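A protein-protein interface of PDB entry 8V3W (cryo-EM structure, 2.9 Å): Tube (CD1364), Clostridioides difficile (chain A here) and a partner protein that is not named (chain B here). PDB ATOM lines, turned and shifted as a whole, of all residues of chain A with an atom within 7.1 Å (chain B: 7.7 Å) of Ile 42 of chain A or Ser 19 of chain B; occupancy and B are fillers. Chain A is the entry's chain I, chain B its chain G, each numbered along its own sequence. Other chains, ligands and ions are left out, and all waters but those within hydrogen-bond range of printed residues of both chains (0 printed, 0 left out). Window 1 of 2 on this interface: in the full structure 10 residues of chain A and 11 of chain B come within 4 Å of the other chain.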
ATOM      1  N   GLU A  39      32.513  -1.998  25.740  1.00  0.00           N
ATOM      2  CA  GLU A  39      31.695  -2.000  24.537  1.00  0.00           C
ATOM      3  C   GLU A  39      31.245  -3.424  24.250  1.00  0.00           C
ATOM      4  O   GLU A  39      32.068  -4.341  24.232  1.00  0.00           O
ATOM      5  CB  GLU A  39      32.465  -1.440  23.343  1.00  0.00           C
ATOM      6  CG  GLU A  39      31.745  -1.615  22.030  1.00  0.00           C
ATOM      7  CD  GLU A  39      32.565  -1.160  20.851  1.00  0.00           C
ATOM      8  OE1 GLU A  39      32.897   0.039  20.783  1.00  0.00           O
ATOM      9  OE2 GLU A  39      32.872  -2.001  19.983  1.00  0.00           O
ATOM     10  N   ASP A  40      29.945  -3.605  24.026  1.00  0.00           N
ATOM     11  CA  ASP A  40      29.403  -4.930  23.756  1.00  0.00           C
ATOM     12  C   ASP A  40      29.734  -5.379  22.340  1.00  0.00           C
ATOM     13  O   ASP A  40      29.659  -4.599  21.390  1.00  0.00           O
ATOM     14  CB  ASP A  40      27.889  -4.933  23.951  1.00  0.00           C
ATOM     15  CG  ASP A  40      27.491  -5.062  25.401  1.00  0.00           C
ATOM     16  OD1 ASP A  40      28.377  -5.314  26.239  1.00  0.00           O
ATOM     17  OD2 ASP A  40      26.291  -4.912  25.705  1.00  0.00           O
ATOM     18  N   ILE A  41      30.088  -6.653  22.200  1.00  0.00           N
ATOM     19  CA  ILE A  41      30.429  -7.243  20.911  1.00  0.00           C
ATOM     20  C   ILE A  41      29.405  -8.324  20.600  1.00  0.00           C
ATOM     21  O   ILE A  41      29.244  -9.276  21.371  1.00  0.00           O
ATOM     22  CB  ILE A  41      31.855  -7.818  20.905  1.00  0.00           C
ATOM     23  CG1 ILE A  41      32.848  -6.765  21.396  1.00  0.00           C
ATOM     24  CG2 ILE A  41      32.226  -8.309  19.524  1.00  0.00           C
ATOM     25  CD1 ILE A  41      33.031  -5.617  20.444  1.00  0.00           C
ATOM     26  N   ILE A  42      28.719  -8.178  19.472  1.00  0.00           N
ATOM     27  CA  ILE A  42      27.692  -9.115  19.037  1.00  0.00           C
ATOM     28  C   ILE A  42      28.046  -9.584  17.634  1.00  0.00           C
ATOM     29  O   ILE A  42      28.305  -8.764  16.748  1.00  0.00           O
ATOM     30  CB  ILE A  42      26.296  -8.472  19.075  1.00  0.00           C
ATOM     31  CG1 ILE A  42      25.847  -8.289  20.523  1.00  0.00           C
ATOM     32  CG2 ILE A  42      25.292  -9.305  18.304  1.00  0.00           C
ATOM     33  CD1 ILE A  42      24.469  -7.715  20.666  1.00  0.00           C
ATOM     34  N   ILE A  43      28.057 -10.898  17.434  1.00  0.00           N
ATOM     35  CA  ILE A  43      28.466 -11.510  16.176  1.00  0.00           C
ATOM     36  C   ILE A  43      27.285 -12.284  15.612  1.00  0.00           C
ATOM     37  O   ILE A  43      26.679 -13.095  16.319  1.00  0.00           O
ATOM     38  CB  ILE A  43      29.683 -12.433  16.369  1.00  0.00           C
ATOM     39  CG1 ILE A  43      30.868 -11.644  16.920  1.00  0.00           C
ATOM     40  CG2 ILE A  43      30.063 -13.102  15.069  1.00  0.00           C
ATOM     41  CD1 ILE A  43      31.981 -12.509  17.431  1.00  0.00           C
ATOM     42  N   ALA A  44      26.961 -12.038  14.346  1.00  0.00           N
ATOM     43  CA  ALA A  44      25.855 -12.745  13.713  1.00  0.00           C
ATOM     44  C   ALA A  44      26.178 -14.228  13.584  1.00  0.00           C
ATOM     45  O   ALA A  44      27.250 -14.603  13.103  1.00  0.00           O
ATOM     46  CB  ALA A  44      25.555 -12.146  12.342  1.00  0.00           C
ATOM     47  N   GLY A  45      25.240 -15.072  14.004  1.00  0.00           N
ATOM     48  CA  GLY A  45      25.441 -16.502  14.017  1.00  0.00           C
ATOM     49  C   GLY A  45      25.931 -17.073  15.330  1.00  0.00           C
ATOM     50  O   GLY A  45      26.002 -18.300  15.462  1.00  0.00           O
ATOM     51  N   GLN A  46      26.271 -16.233  16.301  1.00  0.00           N
ATOM     52  CA  GLN A  46      26.717 -16.673  17.614  1.00  0.00           C
ATOM     53  C   GLN A  46      25.767 -16.137  18.671  1.00  0.00           C
ATOM     54  O   GLN A  46      25.363 -14.973  18.620  1.00  0.00           O
ATOM     55  CB  GLN A  46      28.140 -16.194  17.906  1.00  0.00           C
ATOM     56  CG  GLN A  46      29.117 -16.474  16.791  1.00  0.00           C
ATOM     57  CD  GLN A  46      29.918 -17.730  17.024  1.00  0.00           C
ATOM     58  OE1 GLN A  46      30.157 -18.124  18.164  1.00  0.00           O
ATOM     59  NE2 GLN A  46      30.335 -18.373  15.943  1.00  0.00           N
ATOM     60  N   MET A  47      25.410 -16.990  19.631  1.00  0.00           N
ATOM     61  CA  MET A  47      24.439 -16.601  20.646  1.00  0.00           C
ATOM     62  C   MET A  47      25.051 -15.753  21.755  1.00  0.00           C
ATOM     63  O   MET A  47      24.362 -14.903  22.325  1.00  0.00           O
ATOM     64  CB  MET A  47      23.778 -17.843  21.240  1.00  0.00           C
ATOM     65  CG  MET A  47      22.644 -18.406  20.410  1.00  0.00           C
ATOM     66  SD  MET A  47      21.030 -17.892  21.014  1.00  0.00           S
ATOM     67  CE  MET A  47      20.002 -18.304  19.616  1.00  0.00           C
ATOM     68  N   GLY A  48      26.324 -15.959  22.075  1.00  0.00           N
ATOM     69  CA  GLY A  48      26.939 -15.246  23.175  1.00  0.00           C
ATOM     70  C   GLY A  48      27.258 -13.792  22.865  1.00  0.00           C
ATOM     71  O   GLY A  48      27.236 -13.341  21.724  1.00  0.00           O
ATOM     72  N   THR A  49      27.564 -13.049  23.927  1.00  0.00           N
ATOM     73  CA  THR A  49      27.919 -11.638  23.846  1.00  0.00           C
ATOM     74  C   THR A  49      29.196 -11.404  24.640  1.00  0.00           C
ATOM     75  O   THR A  49      29.322 -11.892  25.766  1.00  0.00           O
ATOM     76  CB  THR A  49      26.782 -10.757  24.379  1.00  0.00           C
ATOM     77  OG1 THR A  49      25.673 -10.807  23.475  1.00  0.00           O
ATOM     78  CG2 THR A  49      27.228  -9.318  24.541  1.00  0.00           C
ATOM     79  N   ASP A  50      30.134 -10.657  24.061  1.00  0.00           N
ATOM     80  CA  ASP A  50      31.431 -10.393  24.668  1.00  0.00           C
ATOM     81  C   ASP A  50      31.661  -8.888  24.742  1.00  0.00           C
ATOM     82  O   ASP A  50      30.848  -8.094  24.268  1.00  0.00           O
ATOM     83  CB  ASP A  50      32.553 -11.077  23.877  1.00  0.00           C
ATOM     84  CG  ASP A  50      33.669 -11.583  24.766  1.00  0.00           C
ATOM     85  OD1 ASP A  50      33.846 -11.036  25.870  1.00  0.00           O
ATOM     86  OD2 ASP A  50      34.359 -12.542  24.368  1.00  0.00           O
ATOM     87  N   MET B   3      33.949 -15.148   6.436  1.00  0.00           N
ATOM     88  CA  MET B   3      33.892 -14.163   5.366  1.00  0.00           C
ATOM     89  C   MET B   3      35.240 -14.090   4.667  1.00  0.00           C
ATOM     90  O   MET B   3      36.271 -13.926   5.323  1.00  0.00           O
ATOM     91  CB  MET B   3      33.490 -12.796   5.913  1.00  0.00           C
ATOM     92  CG  MET B   3      33.085 -11.807   4.848  1.00  0.00           C
ATOM     93  SD  MET B   3      32.619 -10.198   5.498  1.00  0.00           S
ATOM     94  CE  MET B   3      31.190 -10.658   6.451  1.00  0.00           C
ATOM     95  N   VAL B  16      37.270 -10.411  12.481  1.00  0.00           N
ATOM     96  CA  VAL B  16      36.091 -10.246  13.328  1.00  0.00           C
ATOM     97  C   VAL B  16      34.860 -10.234  12.434  1.00  0.00           C
ATOM     98  O   VAL B  16      34.725  -9.361  11.570  1.00  0.00           O
ATOM     99  CB  VAL B  16      36.161  -8.962  14.171  1.00  0.00           C
ATOM    100  CG1 VAL B  16      34.909  -8.815  15.010  1.00  0.00           C
ATOM    101  CG2 VAL B  16      37.385  -8.966  15.062  1.00  0.00           C
ATOM    102  N   PHE B  17      33.958 -11.188  12.652  1.00  0.00           N
ATOM    103  CA  PHE B  17      32.730 -11.297  11.875  1.00  0.00           C
ATOM    104  C   PHE B  17      31.746 -10.204  12.290  1.00  0.00           C
ATOM    105  O   PHE B  17      31.580  -9.941  13.481  1.00  0.00           O
ATOM    106  CB  PHE B  17      32.097 -12.671  12.069  1.00  0.00           C
ATOM    107  CG  PHE B  17      31.165 -13.072  10.967  1.00  0.00           C
ATOM    108  CD1 PHE B  17      31.655 -13.609   9.798  1.00  0.00           C
ATOM    109  CD2 PHE B  17      29.800 -12.916  11.102  1.00  0.00           C
ATOM    110  CE1 PHE B  17      30.807 -13.980   8.785  1.00  0.00           C
ATOM    111  CE2 PHE B  17      28.950 -13.281  10.089  1.00  0.00           C
ATOM    112  CZ  PHE B  17      29.456 -13.814   8.928  1.00  0.00           C
ATOM    113  N   PRO B  18      31.083  -9.558  11.335  1.00  0.00           N
ATOM    114  CA  PRO B  18      30.263  -8.387  11.660  1.00  0.00           C
ATOM    115  C   PRO B  18      28.988  -8.757  12.401  1.00  0.00           C
ATOM    116  O   PRO B  18      28.600  -9.918  12.526  1.00  0.00           O
ATOM    117  CB  PRO B  18      29.950  -7.786  10.291  1.00  0.00           C
ATOM    118  CG  PRO B  18      30.035  -8.924   9.370  1.00  0.00           C
ATOM    119  CD  PRO B  18      31.127  -9.800   9.887  1.00  0.00           C
ATOM    120  N   SER B  19      28.322  -7.717  12.892  1.00  0.00           N
ATOM    121  CA  SER B  19      27.100  -7.898  13.660  1.00  0.00           C
ATOM    122  C   SER B  19      25.909  -8.250  12.778  1.00  0.00           C
ATOM    123  O   SER B  19      24.985  -8.921  13.245  1.00  0.00           O
ATOM    124  CB  SER B  19      26.809  -6.636  14.467  1.00  0.00           C
ATOM    125  OG  SER B  19      25.727  -6.841  15.348  1.00  0.00           O
ATOM    126  N   SER B  20      25.902  -7.807  11.524  1.00  0.00           N
ATOM    127  CA  SER B  20      24.835  -8.162  10.599  1.00  0.00           C
ATOM    128  C   SER B  20      25.301  -7.916   9.172  1.00  0.00           C
ATOM    129  O   SER B  20      26.298  -7.232   8.935  1.00  0.00           O
ATOM    130  CB  SER B  20      23.556  -7.376  10.892  1.00  0.00           C
ATOM    131  OG  SER B  20      23.649  -6.056  10.397  1.00  0.00           O
ATOM    132  N   PHE B  21      24.563  -8.492   8.223  1.00  0.00           N
ATOM    133  CA  PHE B  21      24.804  -8.291   6.800  1.00  0.00           C
ATOM    134  C   PHE B  21      23.484  -8.394   6.047  1.00  0.00           C
ATOM    135  O   PHE B  21      22.620  -9.188   6.418  1.00  0.00           O
ATOM    136  CB  PHE B  21      25.817  -9.304   6.252  1.00  0.00           C
ATOM    137  CG  PHE B  21      25.408 -10.738   6.432  1.00  0.00           C
ATOM    138  CD1 PHE B  21      24.656 -11.385   5.471  1.00  0.00           C
ATOM    139  CD2 PHE B  21      25.812 -11.451   7.544  1.00  0.00           C
ATOM    140  CE1 PHE B  21      24.283 -12.697   5.632  1.00  0.00           C
ATOM    141  CE2 PHE B  21      25.447 -12.771   7.706  1.00  0.00           C
ATOM    142  CZ  PHE B  21      24.682 -13.393   6.748  1.00  0.00           C
ATOM    143  N   ILE B  53      29.483  -3.786   4.601  1.00  0.00           N
ATOM    144  CA  ILE B  53      30.056  -4.477   5.752  1.00  0.00           C
ATOM    145  C   ILE B  53      30.669  -3.459   6.703  1.00  0.00           C
ATOM    146  O   ILE B  53      31.375  -2.544   6.269  1.00  0.00           O
ATOM    147  CB  ILE B  53      31.120  -5.509   5.320  1.00  0.00           C
ATOM    148  CG1 ILE B  53      30.551  -6.461   4.272  1.00  0.00           C
ATOM    149  CG2 ILE B  53      31.657  -6.267   6.525  1.00  0.00           C
ATOM    150  CD1 ILE B  53      29.538  -7.427   4.831  1.00  0.00           C
ATOM    151  N   SER B  54      30.401  -3.618   7.998  1.00  0.00           N
ATOM    152  CA  SER B  54      30.992  -2.787   9.041  1.00  0.00           C
ATOM    153  C   SER B  54      31.536  -3.666  10.154  1.00  0.00           C
ATOM    154  O   SER B  54      30.811  -4.505  10.694  1.00  0.00           O
ATOM    155  CB  SER B  54      29.974  -1.805   9.617  1.00  0.00           C
ATOM    156  OG  SER B  54      29.600  -0.834   8.661  1.00  0.00           O
ATOM    157  N   SER B  55      32.796  -3.460  10.509  1.00  0.00           N
ATOM    158  CA  SER B  55      33.472  -4.207  11.568  1.00  0.00           C
ATOM    159  C   SER B  55      34.762  -3.459  11.887  1.00  0.00           C
ATOM    160  O   SER B  55      34.925  -2.297  11.501  1.00  0.00           O
ATOM    161  CB  SER B  55      33.714  -5.658  11.156  1.00  0.00           C
ATOM    162  OG  SER B  55      34.000  -6.459  12.282  1.00  0.00           O
ATOM    163  N   PHE B  64      37.134 -13.202  21.077  1.00  0.00           N
ATOM    164  CA  PHE B  64      36.069 -13.364  20.098  1.00  0.00           C
ATOM    165  C   PHE B  64      36.567 -13.358  18.659  1.00  0.00           C
ATOM    166  O   PHE B  64      35.744 -13.367  17.739  1.00  0.00           O
ATOM    167  CB  PHE B  64      35.008 -12.270  20.279  1.00  0.00           C
ATOM    168  CG  PHE B  64      35.571 -10.884  20.433  1.00  0.00           C
ATOM    169  CD1 PHE B  64      35.945 -10.147  19.328  1.00  0.00           C
ATOM    170  CD2 PHE B  64      35.721 -10.318  21.684  1.00  0.00           C
ATOM    171  CE1 PHE B  64      36.459  -8.882  19.468  1.00  0.00           C
ATOM    172  CE2 PHE B  64      36.238  -9.053  21.824  1.00  0.00           C
ATOM    173  CZ  PHE B  64      36.601  -8.334  20.714  1.00  0.00           C
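Hydrophobic or aromatic side chains of chain A within 4 Å of the printed part of chain B: Ile 42, Ile 43 and Ala 44.
Of the 11 printed residues of chain B, 4 touch a printed residue of chain A.
Printed residues of chain B that touch a printed residue of chain A: Phe 17, Pro 18, Ser 19 and Phe 64.
Hydrophobic or aromatic side chains of chain B within 4 Å of the printed part of chain A: Phe 17 and Phe 64.
Ile 42 of chain A touches just one residue of chain B: Ser 19 (3.4 Å).
Printed residues of chain B within 4 Å of Ile 43 of chain A: Phe 17 (3.7 Å), Pro 18 (3.98 Å) and Phe 64 (3.9 Å).
Printed residues of chain B within 4 Å of Ala 44 of chain A: Phe 17, Pro 18 and Ser 19.
Printed residues of chain B within 4 Å of Asp 50 of chain A: Phe 64 (3.7 Å).
Met 3 of chain B touches none of the printed residues of chain A.
Of the printed residues of chain A, Phe 17 of chain B touches Ile 43 (3.7 Å) and Ala 44 (3.7 Å).
Of chain A, only Ile 42 (3.4 Å) and Ala 44 (3.4 Å) come within 4 Å of Ser 19 of chain B.
Printed residues of chain A within 4 Å of Phe 64 of chain B: Ile 43 (3.9 Å) and Asp 50 (3.7 Å).
The nearest residue of chain A that does not touch Ser 19 of chain B is Ile 43 of chain A (4.6 Å).
N of Ala 44 of chain A is in hydrogen-bond range of O of Pro 18 of chain B, at 3.2 Å.
N of Ile 41 of chain A is in hydrogen-bond range of O of Asp 50 of chain A (2.6 Å).
Among the printed residues, merely in contact across the chains: Ile 42 of chain A with Ser 19 of chain B (3.4 Å), Ile 43 of chain A with Phe 17 of chain B (3.7 Å), Ile 43 of chain A with Pro 18 of chain B (3.98 Å), Ile 43 of chain A with Phe 64 of chain B (3.9 Å), Ala 44 of chain A with Phe 17 of chain B (3.7 Å), Ala 44 of chain A with Ser 19 of chain B (3.4 Å) and Asp 50 of chain A with Phe 64 of chain B (3.7 Å).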
